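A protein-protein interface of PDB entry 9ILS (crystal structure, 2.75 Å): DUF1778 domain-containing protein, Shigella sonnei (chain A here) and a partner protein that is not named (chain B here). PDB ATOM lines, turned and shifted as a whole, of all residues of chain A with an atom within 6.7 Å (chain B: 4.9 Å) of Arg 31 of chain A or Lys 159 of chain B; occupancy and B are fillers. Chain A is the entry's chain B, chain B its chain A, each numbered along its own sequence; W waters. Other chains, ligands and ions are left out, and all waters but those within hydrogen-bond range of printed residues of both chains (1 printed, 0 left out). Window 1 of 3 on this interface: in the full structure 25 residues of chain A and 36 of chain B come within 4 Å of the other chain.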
ATOM      1  N   GLN A  20      11.939  23.372  24.827  1.00  0.00           N
ATOM      2  CA  GLN A  20      11.561  24.528  24.036  1.00  0.00           C
ATOM      3  C   GLN A  20      10.557  24.160  22.949  1.00  0.00           C
ATOM      4  O   GLN A  20       9.838  25.049  22.475  1.00  0.00           O
ATOM      5  CB  GLN A  20      12.796  25.247  23.471  1.00  0.00           C
ATOM      6  CG  GLN A  20      13.386  24.631  22.252  1.00  0.00           C
ATOM      7  CD  GLN A  20      14.423  25.513  21.514  1.00  0.00           C
ATOM      8  OE1 GLN A  20      14.482  26.748  21.671  1.00  0.00           O
ATOM      9  NE2 GLN A  20      15.227  24.856  20.673  1.00  0.00           N
ATOM     10  N   LEU A  21      10.424  22.867  22.612  1.00  0.00           N
ATOM     11  CA  LEU A  21       9.450  22.366  21.643  1.00  0.00           C
ATOM     12  C   LEU A  21       8.091  22.036  22.258  1.00  0.00           C
ATOM     13  O   LEU A  21       7.057  22.249  21.618  1.00  0.00           O
ATOM     14  CB  LEU A  21      10.011  21.124  20.936  1.00  0.00           C
ATOM     15  CG  LEU A  21       9.431  20.766  19.551  1.00  0.00           C
ATOM     16  CD1 LEU A  21      10.061  21.645  18.495  1.00  0.00           C
ATOM     17  CD2 LEU A  21       9.660  19.308  19.204  1.00  0.00           C
ATOM     18  N   GLU A  22       8.055  21.493  23.475  1.00  0.00           N
ATOM     19  CA  GLU A  22       6.774  21.297  24.146  1.00  0.00           C
ATOM     20  C   GLU A  22       6.256  22.594  24.753  1.00  0.00           C
ATOM     21  O   GLU A  22       5.124  22.627  25.252  1.00  0.00           O
ATOM     22  CB  GLU A  22       6.890  20.277  25.265  1.00  0.00           C
ATOM     23  CG  GLU A  22       8.287  20.230  25.891  1.00  0.00           C
ATOM     24  CD  GLU A  22       8.358  19.354  27.139  1.00  0.00           C
ATOM     25  OE1 GLU A  22       7.765  18.252  27.090  1.00  0.00           O
ATOM     26  OE2 GLU A  22       8.955  19.800  28.175  1.00  0.00           O
ATOM     27  N   ALA A  23       7.069  23.649  24.744  1.00  0.00           N
ATOM     28  CA  ALA A  23       6.634  24.952  25.182  1.00  0.00           C
ATOM     29  C   ALA A  23       5.600  25.514  24.224  1.00  0.00           C
ATOM     30  O   ALA A  23       5.564  25.154  23.045  1.00  0.00           O
ATOM     31  CB  ALA A  23       7.831  25.890  25.288  1.00  0.00           C
ATOM     32  N   PRO A  24       4.734  26.392  24.718  1.00  0.00           N
ATOM     33  CA  PRO A  24       3.771  27.056  23.837  1.00  0.00           C
ATOM     34  C   PRO A  24       4.469  27.796  22.714  1.00  0.00           C
ATOM     35  O   PRO A  24       5.586  28.303  22.848  1.00  0.00           O
ATOM     36  CB  PRO A  24       3.030  28.036  24.758  1.00  0.00           C
ATOM     37  CG  PRO A  24       3.407  27.701  26.114  1.00  0.00           C
ATOM     38  CD  PRO A  24       4.508  26.699  26.131  1.00  0.00           C
ATOM     39  N   VAL A  25       3.769  27.859  21.590  1.00  0.00           N
ATOM     40  CA  VAL A  25       4.349  28.466  20.418  1.00  0.00           C
ATOM     41  C   VAL A  25       4.748  29.895  20.721  1.00  0.00           C
ATOM     42  O   VAL A  25       4.152  30.576  21.563  1.00  0.00           O
ATOM     43  CB  VAL A  25       3.371  28.368  19.246  1.00  0.00           C
ATOM     44  CG1 VAL A  25       4.121  28.648  17.961  1.00  0.00           C
ATOM     45  CG2 VAL A  25       2.833  26.983  19.207  1.00  0.00           C
ATOM     46  N   GLN A  26       5.807  30.317  20.061  1.00  0.00           N
ATOM     47  CA  GLN A  26       6.443  31.612  20.175  1.00  0.00           C
ATOM     48  C   GLN A  26       6.453  32.242  18.797  1.00  0.00           C
ATOM     49  O   GLN A  26       5.949  31.654  17.831  1.00  0.00           O
ATOM     50  CB  GLN A  26       7.854  31.469  20.739  1.00  0.00           C
ATOM     51  CG  GLN A  26       8.054  30.237  21.616  1.00  0.00           C
ATOM     52  CD  GLN A  26       9.521  30.053  22.008  1.00  0.00           C
ATOM     53  OE1 GLN A  26      10.215  31.048  22.251  1.00  0.00           O
ATOM     54  NE2 GLN A  26       9.994  28.793  22.098  1.00  0.00           N
ATOM     55  N   ASN A  27       7.047  33.437  18.710  1.00  0.00           N
ATOM     56  CA  ASN A  27       6.997  34.246  17.485  1.00  0.00           C
ATOM     57  C   ASN A  27       5.608  34.218  16.854  1.00  0.00           C
ATOM     58  O   ASN A  27       5.452  34.169  15.626  1.00  0.00           O
ATOM     59  CB  ASN A  27       8.054  33.801  16.489  1.00  0.00           C
ATOM     60  CG  ASN A  27       8.211  34.773  15.333  1.00  0.00           C
ATOM     61  OD1 ASN A  27       7.467  35.755  15.238  1.00  0.00           O
ATOM     62  ND2 ASN A  27       9.165  34.508  14.452  1.00  0.00           N
ATOM     63  N   ALA A  28       4.582  34.250  17.709  1.00  0.00           N
ATOM     64  CA  ALA A  28       3.216  34.265  17.216  1.00  0.00           C
ATOM     65  C   ALA A  28       2.991  35.390  16.202  1.00  0.00           C
ATOM     66  O   ALA A  28       2.200  35.249  15.256  1.00  0.00           O
ATOM     67  CB  ALA A  28       2.281  34.394  18.414  1.00  0.00           C
ATOM     68  N   GLU A  29       3.728  36.489  16.349  1.00  0.00           N
ATOM     69  CA  GLU A  29       3.540  37.647  15.479  1.00  0.00           C
ATOM     70  C   GLU A  29       3.831  37.315  14.021  1.00  0.00           C
ATOM     71  O   GLU A  29       3.019  37.618  13.139  1.00  0.00           O
ATOM     72  CB  GLU A  29       4.425  38.785  15.985  1.00  0.00           C
ATOM     73  CG  GLU A  29       3.967  39.304  17.343  1.00  0.00           C
ATOM     74  CD  GLU A  29       4.395  38.446  18.539  1.00  0.00           C
ATOM     75  OE1 GLU A  29       5.114  37.424  18.365  1.00  0.00           O
ATOM     76  OE2 GLU A  29       3.935  38.782  19.659  1.00  0.00           O
ATOM     77  N   GLY A  30       4.983  36.693  13.747  1.00  0.00           N
ATOM     78  CA  GLY A  30       5.309  36.315  12.377  1.00  0.00           C
ATOM     79  C   GLY A  30       4.333  35.304  11.807  1.00  0.00           C
ATOM     80  O   GLY A  30       3.765  35.514  10.737  1.00  0.00           O
ATOM     81  N   ARG A  31       4.101  34.206  12.532  1.00  0.00           N
ATOM     82  CA  ARG A  31       3.107  33.217  12.122  1.00  0.00           C
ATOM     83  C   ARG A  31       1.808  33.864  11.673  1.00  0.00           C
ATOM     84  O   ARG A  31       1.173  33.409  10.714  1.00  0.00           O
ATOM     85  CB  ARG A  31       2.835  32.237  13.246  1.00  0.00           C
ATOM     86  CG  ARG A  31       4.064  31.509  13.717  1.00  0.00           C
ATOM     87  CD  ARG A  31       3.808  30.606  14.932  1.00  0.00           C
ATOM     88  NE  ARG A  31       2.873  29.506  14.685  1.00  0.00           N
ATOM     89  CZ  ARG A  31       3.217  28.222  14.645  1.00  0.00           C
ATOM     90  NH1 ARG A  31       4.468  27.833  14.850  1.00  0.00           N
ATOM     91  NH2 ARG A  31       2.281  27.309  14.409  1.00  0.00           N
ATOM     92  N   GLU A  32       1.373  34.914  12.357  1.00  0.00           N
ATOM     93  CA  GLU A  32       0.224  35.631  11.832  1.00  0.00           C
ATOM     94  C   GLU A  32       0.546  36.289  10.520  1.00  0.00           C
ATOM     95  O   GLU A  32      -0.280  36.300   9.605  1.00  0.00           O
ATOM     96  CB  GLU A  32      -0.238  36.670  12.815  1.00  0.00           C
ATOM     97  CG  GLU A  32      -1.347  36.169  13.605  1.00  0.00           C
ATOM     98  CD  GLU A  32      -2.030  37.303  14.252  1.00  0.00           C
ATOM     99  OE1 GLU A  32      -2.480  37.123  15.412  1.00  0.00           O
ATOM    100  OE2 GLU A  32      -2.057  38.382  13.610  1.00  0.00           O
ATOM    101  N   ARG A  33       1.725  36.893  10.428  1.00  0.00           N
ATOM    102  CA  ARG A  33       2.114  37.522   9.182  1.00  0.00           C
ATOM    103  C   ARG A  33       2.202  36.487   8.079  1.00  0.00           C
ATOM    104  O   ARG A  33       1.648  36.684   6.991  1.00  0.00           O
ATOM    105  CB  ARG A  33       3.432  38.254   9.363  1.00  0.00           C
ATOM    106  CG  ARG A  33       3.732  39.188   8.240  1.00  0.00           C
ATOM    107  CD  ARG A  33       4.293  40.480   8.768  1.00  0.00           C
ATOM    108  NE  ARG A  33       5.340  40.246   9.753  1.00  0.00           N
ATOM    109  CZ  ARG A  33       5.391  40.816  10.949  1.00  0.00           C
ATOM    110  NH1 ARG A  33       4.475  41.695  11.333  1.00  0.00           N
ATOM    111  NH2 ARG A  33       6.386  40.500  11.780  1.00  0.00           N
ATOM    112  N   LEU A  34       2.851  35.351   8.345  1.00  0.00           N
ATOM    113  CA  LEU A  34       2.928  34.312   7.317  1.00  0.00           C
ATOM    114  C   LEU A  34       1.552  33.763   6.976  1.00  0.00           C
ATOM    115  O   LEU A  34       1.224  33.574   5.798  1.00  0.00           O
ATOM    116  CB  LEU A  34       3.875  33.189   7.738  1.00  0.00           C
ATOM    117  CG  LEU A  34       4.202  32.225   6.589  1.00  0.00           C
ATOM    118  CD1 LEU A  34       3.214  31.082   6.529  1.00  0.00           C
ATOM    119  CD2 LEU A  34       4.198  32.951   5.246  1.00  0.00           C
ATOM    120  N   MET A  35       0.733  33.500   7.993  1.00  0.00           N
ATOM    121  CA  MET A  35      -0.592  32.939   7.754  1.00  0.00           C
ATOM    122  C   MET A  35      -1.483  33.910   7.013  1.00  0.00           C
ATOM    123  O   MET A  35      -2.536  33.506   6.504  1.00  0.00           O
ATOM    124  CB  MET A  35      -1.218  32.526   9.085  1.00  0.00           C
ATOM    125  CG  MET A  35      -0.787  31.135   9.553  1.00  0.00           C
ATOM    126  SD  MET A  35      -0.651  29.961   8.178  1.00  0.00           S
ATOM    127  CE  MET A  35       0.965  29.241   8.459  1.00  0.00           C
ATOM    128  N   ALA A  36      -1.077  35.180   6.934  1.00  0.00           N
ATOM    129  CA  ALA A  36      -1.832  36.189   6.202  1.00  0.00           C
ATOM    130  C   ALA A  36      -1.408  36.287   4.742  1.00  0.00           C
ATOM    131  O   ALA A  36      -2.256  36.555   3.883  1.00  0.00           O
ATOM    132  CB  ALA A  36      -1.678  37.557   6.879  1.00  0.00           C
ATOM    133  N   LYS B 126       6.357  17.365  14.136  1.00  0.00           N
ATOM    134  CA  LYS B 126       6.389  18.225  15.306  1.00  0.00           C
ATOM    135  C   LYS B 126       6.913  19.627  15.030  1.00  0.00           C
ATOM    136  O   LYS B 126       6.561  20.554  15.765  1.00  0.00           O
ATOM    137  CB  LYS B 126       7.216  17.577  16.416  1.00  0.00           C
ATOM    138  CG  LYS B 126       6.409  16.650  17.322  1.00  0.00           C
ATOM    139  CD  LYS B 126       7.304  16.019  18.423  1.00  0.00           C
ATOM    140  CE  LYS B 126       6.732  16.178  19.855  1.00  0.00           C
ATOM    141  NZ  LYS B 126       7.507  15.522  20.968  1.00  0.00           N
ATOM    142  N   ALA B 127       7.716  19.815  13.993  1.00  0.00           N
ATOM    143  CA  ALA B 127       8.177  21.135  13.600  1.00  0.00           C
ATOM    144  C   ALA B 127       8.824  21.057  12.221  1.00  0.00           C
ATOM    145  O   ALA B 127       9.181  19.979  11.741  1.00  0.00           O
ATOM    146  CB  ALA B 127       9.171  21.702  14.610  1.00  0.00           C
ATOM    147  N   PHE B 144       8.521  35.537  10.038  1.00  0.00           N
ATOM    148  CA  PHE B 144       7.430  34.679   9.568  1.00  0.00           C
ATOM    149  C   PHE B 144       7.250  33.449  10.456  1.00  0.00           C
ATOM    150  O   PHE B 144       6.606  32.479  10.057  1.00  0.00           O
ATOM    151  CB  PHE B 144       7.660  34.292   8.113  1.00  0.00           C
ATOM    152  CG  PHE B 144       7.366  35.398   7.129  1.00  0.00           C
ATOM    153  CD1 PHE B 144       6.070  35.831   6.916  1.00  0.00           C
ATOM    154  CD2 PHE B 144       8.385  35.996   6.421  1.00  0.00           C
ATOM    155  CE1 PHE B 144       5.801  36.845   5.993  1.00  0.00           C
ATOM    156  CE2 PHE B 144       8.127  37.002   5.505  1.00  0.00           C
ATOM    157  CZ  PHE B 144       6.835  37.428   5.293  1.00  0.00           C
ATOM    158  N   GLY B 145       7.783  33.504  11.678  1.00  0.00           N
ATOM    159  CA  GLY B 145       7.377  32.623  12.741  1.00  0.00           C
ATOM    160  C   GLY B 145       8.504  31.808  13.318  1.00  0.00           C
ATOM    161  O   GLY B 145       8.448  31.428  14.496  1.00  0.00           O
ATOM    162  N   PHE B 157      13.464  26.844  14.199  1.00  0.00           N
ATOM    163  CA  PHE B 157      12.345  25.920  14.056  1.00  0.00           C
ATOM    164  C   PHE B 157      11.014  26.665  14.109  1.00  0.00           C
ATOM    165  O   PHE B 157      10.890  27.692  14.782  1.00  0.00           O
ATOM    166  CB  PHE B 157      12.379  24.859  15.130  1.00  0.00           C
ATOM    167  CG  PHE B 157      11.848  25.327  16.414  1.00  0.00           C
ATOM    168  CD1 PHE B 157      12.597  26.179  17.174  1.00  0.00           C
ATOM    169  CD2 PHE B 157      10.623  24.890  16.899  1.00  0.00           C
ATOM    170  CE1 PHE B 157      12.132  26.638  18.392  1.00  0.00           C
ATOM    171  CE2 PHE B 157      10.140  25.341  18.143  1.00  0.00           C
ATOM    172  CZ  PHE B 157      10.908  26.215  18.884  1.00  0.00           C
ATOM    173  N   TYR B 158      10.047  26.141  13.358  1.00  0.00           N
ATOM    174  CA  TYR B 158       8.646  26.545  13.315  1.00  0.00           C
ATOM    175  C   TYR B 158       7.808  25.354  13.777  1.00  0.00           C
ATOM    176  O   TYR B 158       7.618  24.402  13.013  1.00  0.00           O
ATOM    177  CB  TYR B 158       8.263  26.922  11.881  1.00  0.00           C
ATOM    178  CG  TYR B 158       6.877  27.508  11.658  1.00  0.00           C
ATOM    179  CD1 TYR B 158       5.750  26.695  11.572  1.00  0.00           C
ATOM    180  CD2 TYR B 158       6.719  28.866  11.448  1.00  0.00           C
ATOM    181  CE1 TYR B 158       4.488  27.231  11.328  1.00  0.00           C
ATOM    182  CE2 TYR B 158       5.479  29.410  11.200  1.00  0.00           C
ATOM    183  CZ  TYR B 158       4.356  28.594  11.148  1.00  0.00           C
ATOM    184  OH  TYR B 158       3.127  29.179  10.903  1.00  0.00           O
ATOM    185  N   LYS B 159       7.285  25.410  15.005  1.00  0.00           N
ATOM    186  CA  LYS B 159       6.505  24.291  15.546  1.00  0.00           C
ATOM    187  C   LYS B 159       5.197  24.079  14.778  1.00  0.00           C
ATOM    188  O   LYS B 159       4.578  25.028  14.296  1.00  0.00           O
ATOM    189  CB  LYS B 159       6.221  24.530  17.030  1.00  0.00           C
ATOM    190  CG  LYS B 159       5.538  23.404  17.781  1.00  0.00           C
ATOM    191  CD  LYS B 159       5.501  23.713  19.287  1.00  0.00           C
ATOM    192  CE  LYS B 159       4.394  22.927  19.957  1.00  0.00           C
ATOM    193  NZ  LYS B 159       4.672  22.536  21.357  1.00  0.00           N
ATOM    194  N   VAL B 160       4.774  22.822  14.658  1.00  0.00           N
ATOM    195  CA  VAL B 160       3.596  22.448  13.882  1.00  0.00           C
ATOM    196  C   VAL B 160       2.492  22.054  14.855  1.00  0.00           C
ATOM    197  O   VAL B 160       2.692  21.192  15.719  1.00  0.00           O
ATOM    198  CB  VAL B 160       3.907  21.286  12.906  1.00  0.00           C
ATOM    199  CG1 VAL B 160       2.633  20.690  12.299  1.00  0.00           C
ATOM    200  CG2 VAL B 160       4.882  21.701  11.811  1.00  0.00           C
ATOM    201  N   LEU B 161       1.320  22.648  14.692  1.00  0.00           N
ATOM    202  CA  LEU B 161       0.130  22.254  15.434  1.00  0.00           C
ATOM    203  C   LEU B 161      -0.861  21.582  14.492  1.00  0.00           C
ATOM    204  O   LEU B 161      -0.946  21.934  13.307  1.00  0.00           O
ATOM    205  CB  LEU B 161      -0.508  23.476  16.083  1.00  0.00           C
ATOM    206  CG  LEU B 161       0.626  24.296  16.712  1.00  0.00           C
ATOM    207  CD1 LEU B 161       0.280  25.767  16.665  1.00  0.00           C
ATOM    208  CD2 LEU B 161       1.024  23.854  18.135  1.00  0.00           C
HETATM  209  O   HOH W   1       0.873  27.447  11.315  1.00  0.00           O
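NZ of Lys 159 of chain B is in hydrogen-bond range of O of Leu 21 of chain A, at 2.4 Å. The side-chain amide nitrogen (ND2) of Asn 27 of chain A lies close to the backbone carbonyl oxygen (O) of Gly 145 of chain B (3.2 Å). The guanidinium group (NH1) of Arg 31 of chain A lies within hydrogen-bond range of the backbone carbonyl oxygen (O) of Lys 159 of chain B. O of Ala 23 of chain A is in hydrogen-bond range of NZ of Lys 159 of chain B (3.2 Å).
The backbone NH (N) of Gly 30 of chain A lies within hydrogen-bond range of the side-chain amide oxygen (OD1) of Asn 27 of chain A (3.0 Å).
Among the printed residues, pairs that only touch across the chains: Met 35 of chain A with Tyr 158 of chain B (3.3 Å), Arg 31 of chain A with Leu 161 of chain B (3.4 Å), Leu 34 of chain A with Phe 144 of chain B (3.5 Å), Arg 31 of chain A with Tyr 158 of chain B (3.6 Å), Arg 31 of chain A with Gly 145 of chain B (3.6 Å), Leu 21 of chain A with Phe 157 of chain B (3.7 Å), Glu 22 of chain A with Lys 159 of chain B (3.7 Å), Gly 30 of chain A with Phe 144 of chain B (3.7 Å), Val 25 of chain A with Leu 161 of chain B (3.8 Å), Gly 30 of chain A with Gly 145 of chain B (3.8 Å), Arg 31 of chain A with Phe 144 of chain B (3.8 Å), Arg 33 of chain A with Phe 144 of chain B (3.8 Å), Gln 20 of chain A with Phe 157 of chain B (3.9 Å) and Leu 21 of chain A with Ala 127 of chain B (3.99 Å).
Of chain B, only Phe 144, Gly 145, Tyr 158, Lys 159 and Leu 161 come within 4 Å of Arg 31 of chain A. Of chain A, only Leu 21 (2.4 Å), Glu 22 (3.7 Å), Ala 23 (3.2 Å) and Arg 31 (2.9 Å) come within 4 Å of Lys 159 of chain B. Printed residues of chain B within 4 Å of Gln 20 of chain A: Phe 157 (3.9 Å). Of the printed residues of chain B, Val 25 of chain A touches Leu 161.
Printed residues of chain A that touch a printed residue of chain B: Gln 20, Leu 21, Glu 22, Ala 23, Val 25, Asn 27, Gly 30, Arg 31, Arg 33, Leu 34 and Met 35. Among the printed residues, no Asp or Glu carboxylate lies within 4 Å of a Lys or Arg side-chain nitrogen of the other chain.
Water W1 bridges the side-chain hydroxyl (OH) of Tyr 158 of chain B and the guanidinium group (NH2) of Arg 31 of chain A.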
